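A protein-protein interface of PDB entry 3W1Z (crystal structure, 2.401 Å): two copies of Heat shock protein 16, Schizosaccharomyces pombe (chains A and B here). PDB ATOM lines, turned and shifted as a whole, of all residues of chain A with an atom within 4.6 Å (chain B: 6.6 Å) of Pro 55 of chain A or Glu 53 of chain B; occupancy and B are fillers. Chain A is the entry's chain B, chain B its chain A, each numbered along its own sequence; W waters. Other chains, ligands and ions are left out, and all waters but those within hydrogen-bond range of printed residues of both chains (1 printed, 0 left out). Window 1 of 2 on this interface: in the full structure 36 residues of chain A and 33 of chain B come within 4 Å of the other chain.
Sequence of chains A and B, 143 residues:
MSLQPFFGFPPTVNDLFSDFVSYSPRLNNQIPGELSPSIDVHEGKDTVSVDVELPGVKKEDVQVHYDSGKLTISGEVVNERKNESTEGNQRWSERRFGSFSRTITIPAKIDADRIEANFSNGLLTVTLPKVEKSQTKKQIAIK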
ATOM      1  N   GLU A  53      21.334  -5.067  14.757  1.00  0.00           N
ATOM      2  CA  GLU A  53      21.434  -4.706  16.167  1.00  0.00           C
ATOM      3  C   GLU A  53      20.584  -5.619  17.043  1.00  0.00           C
ATOM      4  O   GLU A  53      19.357  -5.636  16.937  1.00  0.00           O
ATOM      5  CB  GLU A  53      21.033  -3.246  16.380  1.00  0.00           C
ATOM      6  CG  GLU A  53      21.997  -2.246  15.765  1.00  0.00           C
ATOM      7  CD  GLU A  53      21.597  -0.809  16.035  1.00  0.00           C
ATOM      8  OE1 GLU A  53      20.438  -0.576  16.437  1.00  0.00           O
ATOM      9  OE2 GLU A  53      22.446   0.089  15.847  1.00  0.00           O
ATOM     10  N   LEU A  54      21.248  -6.378  17.909  1.00  0.00           N
ATOM     11  CA  LEU A  54      20.563  -7.307  18.801  1.00  0.00           C
ATOM     12  C   LEU A  54      21.061  -7.191  20.243  1.00  0.00           C
ATOM     13  O   LEU A  54      21.656  -8.132  20.770  1.00  0.00           O
ATOM     14  CB  LEU A  54      20.753  -8.744  18.307  1.00  0.00           C
ATOM     15  CG  LEU A  54      20.214  -9.086  16.917  1.00  0.00           C
ATOM     16  CD1 LEU A  54      20.602 -10.504  16.522  1.00  0.00           C
ATOM     17  CD2 LEU A  54      18.706  -8.909  16.874  1.00  0.00           C
ATOM     18  N   PRO A  55      20.821  -6.036  20.889  1.00  0.00           N
ATOM     19  CA  PRO A  55      21.256  -5.875  22.281  1.00  0.00           C
ATOM     20  C   PRO A  55      20.430  -6.728  23.240  1.00  0.00           C
ATOM     21  O   PRO A  55      19.209  -6.799  23.106  1.00  0.00           O
ATOM     22  CB  PRO A  55      21.019  -4.387  22.548  1.00  0.00           C
ATOM     23  CG  PRO A  55      19.906  -4.021  21.636  1.00  0.00           C
ATOM     24  CD  PRO A  55      20.100  -4.848  20.396  1.00  0.00           C
ATOM     25  N   GLY A  56      21.095  -7.369  24.195  1.00  0.00           N
ATOM     26  CA  GLY A  56      20.410  -8.177  25.187  1.00  0.00           C
ATOM     27  C   GLY A  56      20.006  -9.546  24.675  1.00  0.00           C
ATOM     28  O   GLY A  56      19.230 -10.255  25.316  1.00  0.00           O
ATOM     29  N   VAL A  57      20.535  -9.921  23.515  1.00  0.00           N
ATOM     30  CA  VAL A  57      20.247 -11.224  22.928  1.00  0.00           C
ATOM     31  C   VAL A  57      21.452 -12.149  23.056  1.00  0.00           C
ATOM     32  O   VAL A  57      22.559 -11.804  22.643  1.00  0.00           O
ATOM     33  CB  VAL A  57      19.863 -11.106  21.440  1.00  0.00           C
ATOM     34  CG1 VAL A  57      19.575 -12.480  20.855  1.00  0.00           C
ATOM     35  CG2 VAL A  57      18.663 -10.190  21.274  1.00  0.00           C
ATOM     36  N   VAL A  77      14.060 -12.027  21.941  1.00  0.00           N
ATOM     37  CA  VAL A  77      14.569 -11.107  22.947  1.00  0.00           C
ATOM     38  C   VAL A  77      13.775 -11.315  24.227  1.00  0.00           C
ATOM     39  O   VAL A  77      12.606 -10.941  24.317  1.00  0.00           O
ATOM     40  CB  VAL A  77      14.452  -9.640  22.502  1.00  0.00           C
ATOM     41  CG1 VAL A  77      15.121  -8.728  23.520  1.00  0.00           C
ATOM     42  CG2 VAL A  77      15.076  -9.451  21.131  1.00  0.00           C
ATOM     43  N   ARG A  95      12.279  -0.598  26.563  1.00  0.00           N
ATOM     44  CA  ARG A  95      12.724  -1.800  25.859  1.00  0.00           C
ATOM     45  C   ARG A  95      11.574  -2.651  25.338  1.00  0.00           C
ATOM     46  O   ARG A  95      10.551  -2.811  25.999  1.00  0.00           O
ATOM     47  CB  ARG A  95      13.657  -2.643  26.737  1.00  0.00           C
ATOM     48  CG  ARG A  95      15.029  -2.025  26.961  1.00  0.00           C
ATOM     49  CD  ARG A  95      15.970  -3.002  27.650  1.00  0.00           C
ATOM     50  NE  ARG A  95      16.341  -4.116  26.782  1.00  0.00           N
ATOM     51  CZ  ARG A  95      16.787  -5.290  27.219  1.00  0.00           C
ATOM     52  NH1 ARG A  95      16.908  -5.515  28.521  1.00  0.00           N
ATOM     53  NH2 ARG A  95      17.102  -6.245  26.356  1.00  0.00           N
ATOM     54  N   GLY A 122      26.271  -7.272  20.976  1.00  0.00           N
ATOM     55  CA  GLY A 122      24.903  -7.042  20.550  1.00  0.00           C
ATOM     56  C   GLY A 122      24.766  -6.747  19.069  1.00  0.00           C
ATOM     57  O   GLY A 122      23.666  -6.486  18.584  1.00  0.00           O
ATOM     58  N   SER B  36      19.022   7.317  20.684  1.00  0.00           N
ATOM     59  CA  SER B  36      18.528   7.309  22.053  1.00  0.00           C
ATOM     60  C   SER B  36      18.583   5.897  22.623  1.00  0.00           C
ATOM     61  O   SER B  36      17.589   5.172  22.549  1.00  0.00           O
ATOM     62  CB  SER B  36      17.095   7.839  22.111  1.00  0.00           C
ATOM     63  OG  SER B  36      16.553   7.692  23.412  1.00  0.00           O
ATOM     64  N   PRO B  37      19.745   5.488  23.161  1.00  0.00           N
ATOM     65  CA  PRO B  37      19.874   4.114  23.660  1.00  0.00           C
ATOM     66  C   PRO B  37      18.763   3.797  24.653  1.00  0.00           C
ATOM     67  O   PRO B  37      18.575   4.526  25.625  1.00  0.00           O
ATOM     68  CB  PRO B  37      21.227   4.131  24.374  1.00  0.00           C
ATOM     69  CG  PRO B  37      21.993   5.220  23.700  1.00  0.00           C
ATOM     70  CD  PRO B  37      20.978   6.269  23.355  1.00  0.00           C
ATOM     71  N   SER B  38      18.043   2.708  24.403  1.00  0.00           N
ATOM     72  CA  SER B  38      16.827   2.406  25.148  1.00  0.00           C
ATOM     73  C   SER B  38      17.120   2.057  26.598  1.00  0.00           C
ATOM     74  O   SER B  38      18.080   1.348  26.898  1.00  0.00           O
ATOM     75  CB  SER B  38      16.041   1.283  24.470  1.00  0.00           C
ATOM     76  OG  SER B  38      15.553   1.697  23.209  1.00  0.00           O
ATOM     77  N   ILE B  39      16.282   2.558  27.497  1.00  0.00           N
ATOM     78  CA  ILE B  39      16.530   2.403  28.923  1.00  0.00           C
ATOM     79  C   ILE B  39      15.345   1.824  29.692  1.00  0.00           C
ATOM     80  O   ILE B  39      14.226   2.335  29.616  1.00  0.00           O
ATOM     81  CB  ILE B  39      16.965   3.741  29.560  1.00  0.00           C
ATOM     82  CG1 ILE B  39      18.346   4.147  29.043  1.00  0.00           C
ATOM     83  CG2 ILE B  39      16.970   3.640  31.078  1.00  0.00           C
ATOM     84  CD1 ILE B  39      18.856   5.446  29.618  1.00  0.00           C
ATOM     85  N   ASP B  40      15.609   0.742  30.419  1.00  0.00           N
ATOM     86  CA  ASP B  40      14.651   0.162  31.347  1.00  0.00           C
ATOM     87  C   ASP B  40      15.126   0.391  32.777  1.00  0.00           C
ATOM     88  O   ASP B  40      16.314   0.281  33.064  1.00  0.00           O
ATOM     89  CB  ASP B  40      14.497  -1.336  31.092  1.00  0.00           C
ATOM     90  CG  ASP B  40      13.463  -1.641  30.032  1.00  0.00           C
ATOM     91  OD1 ASP B  40      13.016  -2.804  29.964  1.00  0.00           O
ATOM     92  OD2 ASP B  40      13.091  -0.719  29.275  1.00  0.00           O
ATOM     93  N   ASP B  51      18.987  -0.765  32.835  1.00  0.00           N
ATOM     94  CA  ASP B  51      19.408  -1.466  31.626  1.00  0.00           C
ATOM     95  C   ASP B  51      19.403  -0.531  30.422  1.00  0.00           C
ATOM     96  O   ASP B  51      18.406   0.126  30.137  1.00  0.00           O
ATOM     97  CB  ASP B  51      18.497  -2.663  31.355  1.00  0.00           C
ATOM     98  CG  ASP B  51      18.635  -3.746  32.402  1.00  0.00           C
ATOM     99  OD1 ASP B  51      19.781  -4.079  32.773  1.00  0.00           O
ATOM    100  OD2 ASP B  51      17.596  -4.266  32.856  1.00  0.00           O
ATOM    101  N   VAL B  52      20.528  -0.479  29.718  1.00  0.00           N
ATOM    102  CA  VAL B  52      20.686   0.391  28.566  1.00  0.00           C
ATOM    103  C   VAL B  52      21.134  -0.425  27.360  1.00  0.00           C
ATOM    104  O   VAL B  52      22.139  -1.132  27.421  1.00  0.00           O
ATOM    105  CB  VAL B  52      21.744   1.482  28.831  1.00  0.00           C
ATOM    106  CG1 VAL B  52      21.567   2.636  27.856  1.00  0.00           C
ATOM    107  CG2 VAL B  52      21.657   1.979  30.266  1.00  0.00           C
ATOM    108  N   GLU B  53      20.386  -0.329  26.266  1.00  0.00           N
ATOM    109  CA  GLU B  53      20.753  -1.025  25.040  1.00  0.00           C
ATOM    110  C   GLU B  53      21.830  -0.255  24.287  1.00  0.00           C
ATOM    111  O   GLU B  53      21.631   0.899  23.910  1.00  0.00           O
ATOM    112  CB  GLU B  53      19.531  -1.224  24.141  1.00  0.00           C
ATOM    113  CG  GLU B  53      18.507  -2.205  24.681  1.00  0.00           C
ATOM    114  CD  GLU B  53      17.334  -2.389  23.739  1.00  0.00           C
ATOM    115  OE1 GLU B  53      17.347  -1.779  22.650  1.00  0.00           O
ATOM    116  OE2 GLU B  53      16.398  -3.137  24.089  1.00  0.00           O
ATOM    117  N   LEU B  54      22.971  -0.901  24.071  1.00  0.00           N
ATOM    118  CA  LEU B  54      24.073  -0.286  23.339  1.00  0.00           C
ATOM    119  C   LEU B  54      24.704  -1.279  22.366  1.00  0.00           C
ATOM    120  O   LEU B  54      25.852  -1.682  22.549  1.00  0.00           O
ATOM    121  CB  LEU B  54      25.136   0.225  24.316  1.00  0.00           C
ATOM    122  CG  LEU B  54      24.752   1.372  25.256  1.00  0.00           C
ATOM    123  CD1 LEU B  54      25.803   1.560  26.339  1.00  0.00           C
ATOM    124  CD2 LEU B  54      24.560   2.657  24.472  1.00  0.00           C
ATOM    125  N   PRO B  55      23.957  -1.678  21.324  1.00  0.00           N
ATOM    126  CA  PRO B  55      24.494  -2.650  20.366  1.00  0.00           C
ATOM    127  C   PRO B  55      25.637  -2.071  19.536  1.00  0.00           C
ATOM    128  O   PRO B  55      25.560  -0.927  19.088  1.00  0.00           O
ATOM    129  CB  PRO B  55      23.290  -2.960  19.472  1.00  0.00           C
ATOM    130  CG  PRO B  55      22.442  -1.739  19.553  1.00  0.00           C
ATOM    131  CD  PRO B  55      22.602  -1.228  20.953  1.00  0.00           C
ATOM    132  N   PHE B 119      28.698  -5.111  31.169  1.00  0.00           N
ATOM    133  CA  PHE B 119      28.352  -4.962  29.760  1.00  0.00           C
ATOM    134  C   PHE B 119      28.358  -6.305  29.038  1.00  0.00           C
ATOM    135  O   PHE B 119      29.413  -6.910  28.850  1.00  0.00           O
ATOM    136  CB  PHE B 119      29.304  -3.980  29.077  1.00  0.00           C
ATOM    137  CG  PHE B 119      28.774  -3.427  27.787  1.00  0.00           C
ATOM    138  CD1 PHE B 119      29.499  -3.543  26.615  1.00  0.00           C
ATOM    139  CD2 PHE B 119      27.543  -2.796  27.747  1.00  0.00           C
ATOM    140  CE1 PHE B 119      29.007  -3.035  25.433  1.00  0.00           C
ATOM    141  CE2 PHE B 119      27.046  -2.287  26.566  1.00  0.00           C
ATOM    142  CZ  PHE B 119      27.779  -2.404  25.406  1.00  0.00           C
ATOM    143  N   SER B 120      27.178  -6.763  28.629  1.00  0.00           N
ATOM    144  CA  SER B 120      27.061  -8.059  27.969  1.00  0.00           C
ATOM    145  C   SER B 120      26.042  -8.038  26.837  1.00  0.00           C
ATOM    146  O   SER B 120      24.913  -7.583  27.021  1.00  0.00           O
ATOM    147  CB  SER B 120      26.686  -9.142  28.983  1.00  0.00           C
ATOM    148  OG  SER B 120      26.364 -10.359  28.332  1.00  0.00           O
ATOM    149  N   ASN B 121      26.448  -8.550  25.677  1.00  0.00           N
ATOM    150  CA  ASN B 121      25.591  -8.611  24.495  1.00  0.00           C
ATOM    151  C   ASN B 121      25.029  -7.254  24.086  1.00  0.00           C
ATOM    152  O   ASN B 121      23.875  -7.152  23.672  1.00  0.00           O
ATOM    153  CB  ASN B 121      24.449  -9.610  24.701  1.00  0.00           C
ATOM    154  CG  ASN B 121      24.945 -11.026  24.907  1.00  0.00           C
ATOM    155  OD1 ASN B 121      25.920 -11.451  24.287  1.00  0.00           O
ATOM    156  ND2 ASN B 121      24.275 -11.766  25.783  1.00  0.00           N
ATOM    157  N   GLY B 122      25.848  -6.216  24.208  1.00  0.00           N
ATOM    158  CA  GLY B 122      25.428  -4.872  23.856  1.00  0.00           C
ATOM    159  C   GLY B 122      24.439  -4.288  24.844  1.00  0.00           C
ATOM    160  O   GLY B 122      23.862  -3.229  24.604  1.00  0.00           O
ATOM    161  N   LEU B 123      24.232  -4.984  25.957  1.00  0.00           N
ATOM    162  CA  LEU B 123      23.364  -4.482  27.013  1.00  0.00           C
ATOM    163  C   LEU B 123      24.172  -4.139  28.258  1.00  0.00           C
ATOM    164  O   LEU B 123      24.857  -4.994  28.827  1.00  0.00           O
ATOM    165  CB  LEU B 123      22.268  -5.493  27.359  1.00  0.00           C
ATOM    166  CG  LEU B 123      21.181  -4.956  28.294  1.00  0.00           C
ATOM    167  CD1 LEU B 123      20.301  -3.945  27.568  1.00  0.00           C
ATOM    168  CD2 LEU B 123      20.344  -6.083  28.886  1.00  0.00           C
ATOM    169  N   LEU B 124      24.092  -2.876  28.661  1.00  0.00           N
ATOM    170  CA  LEU B 124      24.733  -2.413  29.883  1.00  0.00           C
ATOM    171  C   LEU B 124      23.743  -2.469  31.034  1.00  0.00           C
ATOM    172  O   LEU B 124      22.632  -1.969  30.929  1.00  0.00           O
ATOM    173  CB  LEU B 124      25.238  -0.979  29.711  1.00  0.00           C
ATOM    174  CG  LEU B 124      25.707  -0.282  30.990  1.00  0.00           C
ATOM    175  CD1 LEU B 124      26.944  -0.963  31.556  1.00  0.00           C
ATOM    176  CD2 LEU B 124      25.967   1.195  30.738  1.00  0.00           C
HETATM  177  O   HOH W   1      26.943 -10.190  21.372  1.00  0.00           O
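N of Gly 122 of chain A lies close to N of Gly 122 of chain B. The side-chain carboxylate (OE2) of Glu 53 of chain B lies within salt-bridge range of the guanidinium group (NE) of Arg 95 of chain A (2.9 Å). The side-chain carboxylate (OD2) of Asp 40 of chain B is in hydrogen-bond range of the backbone NH (N) of Arg 95 of chain A (2.8 Å). O of Asn 121 of chain B is in hydrogen-bond range of N of Gly 56 of chain A (2.8 Å).
N of Leu 54 of chain A is in hydrogen-bond range of O of Gly 122 of chain A (2.5 Å). N of Leu 54 of chain B sits at hydrogen-bond distance from O of Gly 122 of chain B, at 2.5 Å. The backbone NH (N) of Asp 40 of chain B lies within hydrogen-bond range of the backbone carbonyl oxygen (O) of Asp 51 of chain B, at 2.9 Å. O of Ser 38 of chain B lies within hydrogen-bond range of N of Glu 53 of chain B, at 2.9 Å.
Among the printed residues, pairs that only touch across the chains: Pro 55 of chain A with Asn 121 of chain B, Gly 122 of chain A with Asn 121 of chain B, Val 57 of chain A with Asn 121 of chain B, Arg 95 of chain A with Leu 123 of chain B, Pro 55 of chain A with Glu 53 of chain B, Gly 122 of chain A with Pro 55 of chain B, Pro 55 of chain A with Gly 122 of chain B, Glu 53 of chain A with Pro 55 of chain B, Leu 54 of chain A with Asn 121 of chain B, Pro 55 of chain A with Pro 55 of chain B and Gly 56 of chain A with Leu 123 of chain B.
Of the printed residues of chain B, Leu 54 of chain A touches Asn 121 (3.8 Å). Pro 55 of chain A touches just these residues of chain B: Glu 53, Pro 55, Asn 121 and Gly 122. Of the printed residues of chain B, Gly 56 of chain A touches Asn 121 (2.8 Å) and Leu 123 (3.9 Å). Val 77 of chain A touches none of the printed residues of chain B. Of the printed residues of chain A, Asp 40 of chain B touches Arg 95. Glu 53 of chain B touches two residues of chain A. Of the printed residues of chain A, Pro 55 of chain B touches Glu 53 (3.7 Å), Pro 55 (3.8 Å) and Gly 122 (3.7 Å). Of the printed residues of chain A, Leu 123 of chain B touches Gly 56 and Arg 95. The nearest printed residue of chain A that does not touch Glu 53 of chain B is Val 77 of chain A (5.8 Å). The nearest printed residue of chain A that does not touch Leu 123 of chain B is Pro 55 of chain A (4.7 Å).
Printed residues of chain A that touch a printed residue of chain B: Glu 53, Leu 54, Pro 55, Gly 56, Val 57, Arg 95 and Gly 122. Hydrophobic or aromatic side chains of chain A that line the printed part of chain B: Pro 55. Of the 16 printed residues of chain B, 6 touch a printed residue of chain A. Printed residues of chain B that touch a printed residue of chain A: Asp 40, Glu 53, Pro 55, Asn 121, Gly 122 and Leu 123. Hydrophobic or aromatic side chains of chain B that line the printed part of chain A: Pro 55 and Leu 123. Along chain B the printed residues that touch a printed residue of chain A span positions 40 to 123. Among the printed residues, Asp or Glu carboxylates within 4 Å of a Lys or Arg side-chain nitrogen of the other chain: Arg 95 of chain A with Glu 53 of chain B (2.9 Å).
Glu 53 of chain A touches Pro 55 of chain B, and with the chains exchanged Pro 55 of chain A touches Glu 53 of chain B. Pro 55 of chain B touches its own counterpart, Pro 55 of chain A. Pro 55 of chain A touches Gly 122 of chain B, and with the chains exchanged Gly 122 of chain A touches Pro 55 of chain B. Gly 122 of chain A touches its own counterpart, Gly 122 of chain B. Of the 15 pairs that touch across the chains among the printed residues, 6 have their exchanged pair printed and touching as well.
Water W1 bridges the backbone NH of Gly 122 of chain A (3.0 Å) and the side-chain amide oxygen of Asn 121 of chain B (3.3 Å).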
